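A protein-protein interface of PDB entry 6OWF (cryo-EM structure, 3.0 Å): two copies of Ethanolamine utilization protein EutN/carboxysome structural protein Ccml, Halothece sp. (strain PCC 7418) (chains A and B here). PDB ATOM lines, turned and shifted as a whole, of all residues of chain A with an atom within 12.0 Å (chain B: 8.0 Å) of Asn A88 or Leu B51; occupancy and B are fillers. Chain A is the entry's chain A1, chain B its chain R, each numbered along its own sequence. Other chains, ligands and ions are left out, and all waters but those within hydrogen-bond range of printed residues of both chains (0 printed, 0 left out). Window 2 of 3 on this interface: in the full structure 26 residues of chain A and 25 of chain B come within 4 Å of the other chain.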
ATOM      1  N   MET A   3       4.462  -0.077 -34.651  1.00  0.00           N
ATOM      2  CA  MET A   3       4.413  -1.372 -33.994  1.00  0.00           C
ATOM      3  C   MET A   3       4.667  -2.447 -35.037  1.00  0.00           C
ATOM      4  O   MET A   3       4.086  -2.413 -36.124  1.00  0.00           O
ATOM      5  CB  MET A   3       3.065  -1.601 -33.312  1.00  0.00           C
ATOM      6  CG  MET A   3       2.593  -0.450 -32.452  1.00  0.00           C
ATOM      7  SD  MET A   3       1.210  -0.924 -31.403  1.00  0.00           S
ATOM      8  CE  MET A   3       0.061  -1.536 -32.626  1.00  0.00           C
ATOM      9  N   ALA A  32      -3.387  -1.245 -36.235  1.00  0.00           N
ATOM     10  CA  ALA A  32      -3.789  -0.798 -34.905  1.00  0.00           C
ATOM     11  C   ALA A  32      -4.513  -1.903 -34.147  1.00  0.00           C
ATOM     12  O   ALA A  32      -4.465  -1.957 -32.913  1.00  0.00           O
ATOM     13  CB  ALA A  32      -4.667   0.448 -35.011  1.00  0.00           C
ATOM     14  N   ASN A  33      -5.191  -2.796 -34.871  1.00  0.00           N
ATOM     15  CA  ASN A  33      -5.843  -3.928 -34.226  1.00  0.00           C
ATOM     16  C   ASN A  33      -4.809  -4.962 -33.796  1.00  0.00           C
ATOM     17  O   ASN A  33      -4.884  -5.488 -32.680  1.00  0.00           O
ATOM     18  CB  ASN A  33      -6.880  -4.522 -35.193  1.00  0.00           C
ATOM     19  CG  ASN A  33      -7.837  -5.535 -34.541  1.00  0.00           C
ATOM     20  OD1 ASN A  33      -7.489  -6.286 -33.632  1.00  0.00           O
ATOM     21  ND2 ASN A  33      -9.069  -5.547 -35.033  1.00  0.00           N
ATOM     22  N   THR A  84       2.630  -3.367 -23.339  1.00  0.00           N
ATOM     23  CA  THR A  84       1.178  -3.358 -23.428  1.00  0.00           C
ATOM     24  C   THR A  84       0.716  -2.232 -24.340  1.00  0.00           C
ATOM     25  O   THR A  84       1.335  -1.166 -24.392  1.00  0.00           O
ATOM     26  CB  THR A  84       0.529  -3.230 -22.043  1.00  0.00           C
ATOM     27  OG1 THR A  84      -0.885  -3.042 -22.185  1.00  0.00           O
ATOM     28  CG2 THR A  84       1.128  -2.087 -21.260  1.00  0.00           C
ATOM     29  N   VAL A  85      -0.353  -2.497 -25.085  1.00  0.00           N
ATOM     30  CA  VAL A  85      -1.053  -1.493 -25.875  1.00  0.00           C
ATOM     31  C   VAL A  85      -2.467  -1.390 -25.331  1.00  0.00           C
ATOM     32  O   VAL A  85      -3.151  -2.408 -25.180  1.00  0.00           O
ATOM     33  CB  VAL A  85      -1.071  -1.846 -27.373  1.00  0.00           C
ATOM     34  CG1 VAL A  85      -1.727  -0.739 -28.165  1.00  0.00           C
ATOM     35  CG2 VAL A  85       0.326  -2.086 -27.875  1.00  0.00           C
ATOM     36  N   THR A  86      -2.898  -0.174 -25.019  1.00  0.00           N
ATOM     37  CA  THR A  86      -4.220   0.067 -24.461  1.00  0.00           C
ATOM     38  C   THR A  86      -4.978   0.978 -25.414  1.00  0.00           C
ATOM     39  O   THR A  86      -4.738   2.186 -25.439  1.00  0.00           O
ATOM     40  CB  THR A  86      -4.121   0.693 -23.069  1.00  0.00           C
ATOM     41  OG1 THR A  86      -3.407  -0.194 -22.201  1.00  0.00           O
ATOM     42  CG2 THR A  86      -5.505   0.927 -22.489  1.00  0.00           C
ATOM     43  N   VAL A  87      -5.885   0.399 -26.195  1.00  0.00           N
ATOM     44  CA  VAL A  87      -6.659   1.129 -27.191  1.00  0.00           C
ATOM     45  C   VAL A  87      -8.061   1.321 -26.642  1.00  0.00           C
ATOM     46  O   VAL A  87      -8.717   0.339 -26.275  1.00  0.00           O
ATOM     47  CB  VAL A  87      -6.712   0.385 -28.532  1.00  0.00           C
ATOM     48  CG1 VAL A  87      -7.427   1.222 -29.577  1.00  0.00           C
ATOM     49  CG2 VAL A  87      -5.328   0.020 -28.984  1.00  0.00           C
ATOM     50  N   ASN A  88      -8.515   2.582 -26.600  1.00  0.00           N
ATOM     51  CA  ASN A  88      -9.851   2.972 -26.126  1.00  0.00           C
ATOM     52  C   ASN A  88     -10.103   2.498 -24.697  1.00  0.00           C
ATOM     53  O   ASN A  88     -11.156   1.937 -24.387  1.00  0.00           O
ATOM     54  CB  ASN A  88     -10.951   2.478 -27.072  1.00  0.00           C
ATOM     55  CG  ASN A  88     -12.211   3.314 -26.994  1.00  0.00           C
ATOM     56  OD1 ASN A  88     -12.174   4.483 -26.609  1.00  0.00           O
ATOM     57  ND2 ASN A  88     -13.338   2.717 -27.360  1.00  0.00           N
ATOM     58  N   ASN A  89      -9.109   2.710 -23.834  1.00  0.00           N
ATOM     59  CA  ASN A  89      -9.095   2.364 -22.413  1.00  0.00           C
ATOM     60  C   ASN A  89      -9.337   0.882 -22.137  1.00  0.00           C
ATOM     61  O   ASN A  89      -9.832   0.535 -21.059  1.00  0.00           O
ATOM     62  CB  ASN A  89     -10.098   3.211 -21.618  1.00  0.00           C
ATOM     63  CG  ASN A  89      -9.440   4.369 -20.901  1.00  0.00           C
ATOM     64  OD1 ASN A  89      -8.496   4.182 -20.136  1.00  0.00           O
ATOM     65  ND2 ASN A  89      -9.935   5.576 -21.147  1.00  0.00           N
ATOM     66  N   ARG A  90      -8.997  -0.006 -23.069  1.00  0.00           N
ATOM     67  CA  ARG A  90      -9.026  -1.441 -22.824  1.00  0.00           C
ATOM     68  C   ARG A  90      -7.761  -2.065 -23.397  1.00  0.00           C
ATOM     69  O   ARG A  90      -7.194  -1.553 -24.368  1.00  0.00           O
ATOM     70  CB  ARG A  90     -10.281  -2.100 -23.412  1.00  0.00           C
ATOM     71  CG  ARG A  90     -10.378  -2.104 -24.921  1.00  0.00           C
ATOM     72  CD  ARG A  90     -11.397  -3.119 -25.406  1.00  0.00           C
ATOM     73  NE  ARG A  90     -12.765  -2.725 -25.083  1.00  0.00           N
ATOM     74  CZ  ARG A  90     -13.843  -3.406 -25.457  1.00  0.00           C
ATOM     75  NH1 ARG A  90     -15.052  -2.977 -25.121  1.00  0.00           N
ATOM     76  NH2 ARG A  90     -13.714  -4.518 -26.166  1.00  0.00           N
ATOM     77  N   ARG A  91      -7.321  -3.159 -22.783  1.00  0.00           N
ATOM     78  CA  ARG A  91      -6.021  -3.742 -23.084  1.00  0.00           C
ATOM     79  C   ARG A  91      -6.061  -4.487 -24.410  1.00  0.00           C
ATOM     80  O   ARG A  91      -7.090  -5.056 -24.783  1.00  0.00           O
ATOM     81  CB  ARG A  91      -5.616  -4.682 -21.953  1.00  0.00           C
ATOM     82  CG  ARG A  91      -4.136  -4.951 -21.814  1.00  0.00           C
ATOM     83  CD  ARG A  91      -3.852  -5.558 -20.444  1.00  0.00           C
ATOM     84  NE  ARG A  91      -4.941  -6.423 -19.994  1.00  0.00           N
ATOM     85  CZ  ARG A  91      -4.913  -7.753 -20.017  1.00  0.00           C
ATOM     86  NH1 ARG A  91      -3.845  -8.396 -20.464  1.00  0.00           N
ATOM     87  NH2 ARG A  91      -5.960  -8.444 -19.588  1.00  0.00           N
ATOM     88  N   LEU A  92      -4.939  -4.478 -25.128  1.00  0.00           N
ATOM     89  CA  LEU A  92      -4.844  -5.120 -26.433  1.00  0.00           C
ATOM     90  C   LEU A  92      -3.678  -6.094 -26.539  1.00  0.00           C
ATOM     91  O   LEU A  92      -3.812  -7.143 -27.175  1.00  0.00           O
ATOM     92  CB  LEU A  92      -4.716  -4.058 -27.527  1.00  0.00           C
ATOM     93  CG  LEU A  92      -5.106  -4.454 -28.947  1.00  0.00           C
ATOM     94  CD1 LEU A  92      -6.613  -4.392 -29.103  1.00  0.00           C
ATOM     95  CD2 LEU A  92      -4.416  -3.551 -29.951  1.00  0.00           C
ATOM     96  N   TYR A  93      -2.532  -5.769 -25.940  1.00  0.00           N
ATOM     97  CA  TYR A  93      -1.345  -6.622 -25.960  1.00  0.00           C
ATOM     98  C   TYR A  93      -0.793  -6.749 -24.536  1.00  0.00           C
ATOM     99  O   TYR A  93       0.362  -6.447 -24.250  1.00  0.00           O
ATOM    100  CB  TYR A  93      -0.284  -6.107 -26.937  1.00  0.00           C
ATOM    101  CG  TYR A  93       0.873  -7.068 -27.138  1.00  0.00           C
ATOM    102  CD1 TYR A  93       0.659  -8.352 -27.615  1.00  0.00           C
ATOM    103  CD2 TYR A  93       2.171  -6.698 -26.812  1.00  0.00           C
ATOM    104  CE1 TYR A  93       1.709  -9.232 -27.782  1.00  0.00           C
ATOM    105  CE2 TYR A  93       3.222  -7.568 -26.971  1.00  0.00           C
ATOM    106  CZ  TYR A  93       2.988  -8.832 -27.458  1.00  0.00           C
ATOM    107  OH  TYR A  93       4.039  -9.702 -27.622  1.00  0.00           O
ATOM    108  N   LYS B   5      -5.903  11.299 -34.702  1.00  0.00           N
ATOM    109  CA  LYS B   5      -6.749  11.120 -33.535  1.00  0.00           C
ATOM    110  C   LYS B   5      -6.073  10.172 -32.559  1.00  0.00           C
ATOM    111  O   LYS B   5      -5.625   9.090 -32.947  1.00  0.00           O
ATOM    112  CB  LYS B   5      -8.119  10.572 -33.933  1.00  0.00           C
ATOM    113  CG  LYS B   5      -9.113  10.525 -32.802  1.00  0.00           C
ATOM    114  CD  LYS B   5     -10.467  10.053 -33.284  1.00  0.00           C
ATOM    115  CE  LYS B   5     -11.465   9.982 -32.140  1.00  0.00           C
ATOM    116  NZ  LYS B   5     -12.794   9.490 -32.589  1.00  0.00           N
ATOM    117  N   VAL B   6      -6.002  10.576 -31.292  1.00  0.00           N
ATOM    118  CA  VAL B   6      -5.343   9.771 -30.271  1.00  0.00           C
ATOM    119  C   VAL B   6      -6.220   8.582 -29.922  1.00  0.00           C
ATOM    120  O   VAL B   6      -7.160   8.700 -29.131  1.00  0.00           O
ATOM    121  CB  VAL B   6      -5.034  10.595 -29.012  1.00  0.00           C
ATOM    122  CG1 VAL B   6      -4.103   9.827 -28.106  1.00  0.00           C
ATOM    123  CG2 VAL B   6      -4.441  11.932 -29.386  1.00  0.00           C
ATOM    124  N   CYS B   7      -5.914   7.423 -30.504  1.00  0.00           N
ATOM    125  CA  CYS B   7      -6.731   6.243 -30.256  1.00  0.00           C
ATOM    126  C   CYS B   7      -6.362   5.575 -28.942  1.00  0.00           C
ATOM    127  O   CYS B   7      -7.245   5.160 -28.184  1.00  0.00           O
ATOM    128  CB  CYS B   7      -6.605   5.258 -31.415  1.00  0.00           C
ATOM    129  SG  CYS B   7      -7.826   5.523 -32.716  1.00  0.00           S
ATOM    130  N   GLY B   8      -5.074   5.463 -28.649  1.00  0.00           N
ATOM    131  CA  GLY B   8      -4.697   4.710 -27.471  1.00  0.00           C
ATOM    132  C   GLY B   8      -3.296   5.023 -27.003  1.00  0.00           C
ATOM    133  O   GLY B   8      -2.731   6.076 -27.300  1.00  0.00           O
ATOM    134  N   THR B   9      -2.747   4.082 -26.245  1.00  0.00           N
ATOM    135  CA  THR B   9      -1.473   4.246 -25.567  1.00  0.00           C
ATOM    136  C   THR B   9      -0.626   2.996 -25.775  1.00  0.00           C
ATOM    137  O   THR B   9      -1.142   1.877 -25.735  1.00  0.00           O
ATOM    138  CB  THR B   9      -1.720   4.504 -24.075  1.00  0.00           C
ATOM    139  OG1 THR B   9      -2.526   5.678 -23.928  1.00  0.00           O
ATOM    140  CG2 THR B   9      -0.441   4.729 -23.331  1.00  0.00           C
ATOM    141  N   LYS B  23       6.454   9.647 -23.387  1.00  0.00           N
ATOM    142  CA  LYS B  23       5.086   9.156 -23.433  1.00  0.00           C
ATOM    143  C   LYS B  23       4.743   8.768 -24.864  1.00  0.00           C
ATOM    144  O   LYS B  23       4.735   9.620 -25.756  1.00  0.00           O
ATOM    145  CB  LYS B  23       4.140  10.230 -22.907  1.00  0.00           C
ATOM    146  CG  LYS B  23       2.678   9.986 -23.159  1.00  0.00           C
ATOM    147  CD  LYS B  23       1.883  11.197 -22.718  1.00  0.00           C
ATOM    148  CE  LYS B  23       0.396  10.982 -22.885  1.00  0.00           C
ATOM    149  NZ  LYS B  23      -0.352  12.229 -22.586  1.00  0.00           N
ATOM    150  N   LEU B  25       2.158   7.546 -27.544  1.00  0.00           N
ATOM    151  CA  LEU B  25       0.744   7.483 -27.868  1.00  0.00           C
ATOM    152  C   LEU B  25       0.507   6.485 -28.988  1.00  0.00           C
ATOM    153  O   LEU B  25       1.433   5.883 -29.526  1.00  0.00           O
ATOM    154  CB  LEU B  25       0.217   8.856 -28.279  1.00  0.00           C
ATOM    155  CG  LEU B  25       0.082   9.896 -27.180  1.00  0.00           C
ATOM    156  CD1 LEU B  25      -0.580  11.119 -27.759  1.00  0.00           C
ATOM    157  CD2 LEU B  25      -0.733   9.335 -26.036  1.00  0.00           C
ATOM    158  N   LEU B  26      -0.760   6.309 -29.331  1.00  0.00           N
ATOM    159  CA  LEU B  26      -1.156   5.509 -30.480  1.00  0.00           C
ATOM    160  C   LEU B  26      -2.170   6.323 -31.265  1.00  0.00           C
ATOM    161  O   LEU B  26      -3.356   6.341 -30.926  1.00  0.00           O
ATOM    162  CB  LEU B  26      -1.730   4.164 -30.054  1.00  0.00           C
ATOM    163  CG  LEU B  26      -2.132   3.251 -31.205  1.00  0.00           C
ATOM    164  CD1 LEU B  26      -0.935   2.959 -32.050  1.00  0.00           C
ATOM    165  CD2 LEU B  26      -2.698   1.973 -30.671  1.00  0.00           C
ATOM    166  N   GLY B  48       0.387  17.459 -23.435  1.00  0.00           N
ATOM    167  CA  GLY B  48      -0.473  16.408 -22.923  1.00  0.00           C
ATOM    168  C   GLY B  48      -1.742  16.182 -23.716  1.00  0.00           C
ATOM    169  O   GLY B  48      -2.685  16.973 -23.635  1.00  0.00           O
ATOM    170  N   ALA B  49      -1.778  15.093 -24.478  1.00  0.00           N
ATOM    171  CA  ALA B  49      -2.901  14.763 -25.342  1.00  0.00           C
ATOM    172  C   ALA B  49      -3.681  13.607 -24.739  1.00  0.00           C
ATOM    173  O   ALA B  49      -3.107  12.561 -24.421  1.00  0.00           O
ATOM    174  CB  ALA B  49      -2.425  14.403 -26.749  1.00  0.00           C
ATOM    175  N   GLY B  50      -4.987  13.795 -24.590  1.00  0.00           N
ATOM    176  CA  GLY B  50      -5.859  12.777 -24.030  1.00  0.00           C
ATOM    177  C   GLY B  50      -6.425  11.889 -25.123  1.00  0.00           C
ATOM    178  O   GLY B  50      -6.241  12.152 -26.308  1.00  0.00           O
ATOM    179  N   LEU B  51      -7.107  10.825 -24.706  1.00  0.00           N
ATOM    180  CA  LEU B  51      -7.723   9.895 -25.641  1.00  0.00           C
ATOM    181  C   LEU B  51      -8.890  10.562 -26.355  1.00  0.00           C
ATOM    182  O   LEU B  51      -9.719  11.216 -25.720  1.00  0.00           O
ATOM    183  CB  LEU B  51      -8.183   8.634 -24.908  1.00  0.00           C
ATOM    184  CG  LEU B  51      -8.527   7.383 -25.717  1.00  0.00           C
ATOM    185  CD1 LEU B  51      -8.046   6.167 -24.961  1.00  0.00           C
ATOM    186  CD2 LEU B  51     -10.019   7.271 -25.973  1.00  0.00           C
ATOM    187  N   GLY B  52      -8.960  10.403 -27.673  1.00  0.00           N
ATOM    188  CA  GLY B  52      -9.996  11.027 -28.460  1.00  0.00           C
ATOM    189  C   GLY B  52      -9.653  12.402 -28.980  1.00  0.00           C
ATOM    190  O   GLY B  52     -10.445  12.973 -29.739  1.00  0.00           O
ATOM    191  N   GLU B  53      -8.512  12.956 -28.589  1.00  0.00           N
ATOM    192  CA  GLU B  53      -8.094  14.262 -29.065  1.00  0.00           C
ATOM    193  C   GLU B  53      -7.696  14.198 -30.529  1.00  0.00           C
ATOM    194  O   GLU B  53      -7.258  13.160 -31.024  1.00  0.00           O
ATOM    195  CB  GLU B  53      -6.897  14.780 -28.274  1.00  0.00           C
ATOM    196  CG  GLU B  53      -7.187  15.290 -26.886  1.00  0.00           C
ATOM    197  CD  GLU B  53      -7.786  16.672 -26.885  1.00  0.00           C
ATOM    198  OE1 GLU B  53      -8.344  17.069 -25.844  1.00  0.00           O
ATOM    199  OE2 GLU B  53      -7.758  17.347 -27.932  1.00  0.00           O
ATOM    200  N   TRP B  54      -7.842  15.323 -31.217  1.00  0.00           N
ATOM    201  CA  TRP B  54      -7.222  15.504 -32.520  1.00  0.00           C
ATOM    202  C   TRP B  54      -5.914  16.249 -32.320  1.00  0.00           C
ATOM    203  O   TRP B  54      -5.893  17.311 -31.694  1.00  0.00           O
ATOM    204  CB  TRP B  54      -8.128  16.283 -33.470  1.00  0.00           C
ATOM    205  CG  TRP B  54      -9.282  15.507 -34.019  1.00  0.00           C
ATOM    206  CD1 TRP B  54      -9.843  14.380 -33.497  1.00  0.00           C
ATOM    207  CD2 TRP B  54     -10.026  15.813 -35.200  1.00  0.00           C
ATOM    208  NE1 TRP B  54     -10.887  13.964 -34.282  1.00  0.00           N
ATOM    209  CE2 TRP B  54     -11.019  14.829 -35.337  1.00  0.00           C
ATOM    210  CE3 TRP B  54      -9.945  16.827 -36.159  1.00  0.00           C
ATOM    211  CZ2 TRP B  54     -11.925  14.827 -36.391  1.00  0.00           C
ATOM    212  CZ3 TRP B  54     -10.844  16.822 -37.205  1.00  0.00           C
ATOM    213  CH2 TRP B  54     -11.821  15.831 -37.313  1.00  0.00           C
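Val A85 touches Thr B9.
Leu B26 touches Val A85 (CD2 to CG1, 3.8 Å).
Thr A86 touches Gly B8 (O to CA, 3.2 Å).
CD2 of Leu B26 touches CG2 of Val A87, 3.7 Å away.
Asn A88 touches Leu B51 (OD1 to CD2, 3.6 Å).
Leu B51 touches Asn A89.
Leu B51 touches just these residues of chain A: Asn A88 and Asn A89.
No residue of chain A comes within 4 Å of Val B6.
Printed residues of chain A within 4 Å of Gly B8: Thr A86 (3.2 Å).
Ala B49 touches none of the printed residues of chain A.
No residue of chain A comes within 4 Å of Gly B50.
No residue of chain A comes within 4 Å of Glu B53.
Printed residues of chain B within 4 Å of Val A85: Thr B9 and Leu B26.
Of the printed residues of chain A, Leu B26 touches Val A85 (3.8 Å) and Val A87 (3.7 Å).
Of the printed residues of chain B, Asn A89 touches Leu B51.
Printed residues of chain B within 4 Å of Val A87: Leu B26 (3.7 Å).
Of the printed residues of chain B, Thr A86 touches Gly B8 (3.2 Å) and Thr B9 (2.8 Å).
The nearest residue of chain B that does not touch Asn A88 is Gly B8 (4.5 Å).
The nearest residue of chain A that does not touch Leu B51 is Val A87 (5.1 Å).
No position is printed for both chains.
Of the 8 pairs that touch across the chains among the printed residues, none has its exchanged pair printed and touching as well.
O of Val A85 lies within hydrogen-bond range of N of Leu A92 (2.7 Å).
The backbone carbonyl oxygen of Gly B8 sits at hydrogen-bond distance from the backbone NH of Leu B26, at 2.8 Å.
The backbone NH (N) of Cys B7 lies within hydrogen-bond range of the backbone carbonyl oxygen (O) of Leu B26 (2.8 Å).
Of the 13 printed residues of chain A, 5 touch a printed residue of chain B.
Printed residues of chain A that touch a printed residue of chain B: Val A85, Thr A86, Val A87, Asn A88 and Asn A89.
The backbone NH of Thr A86 lies within hydrogen-bond range of the backbone carbonyl oxygen of Thr B9, 2.8 Å away.
N of Asn A88 is in hydrogen-bond range of O of Cys B7.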
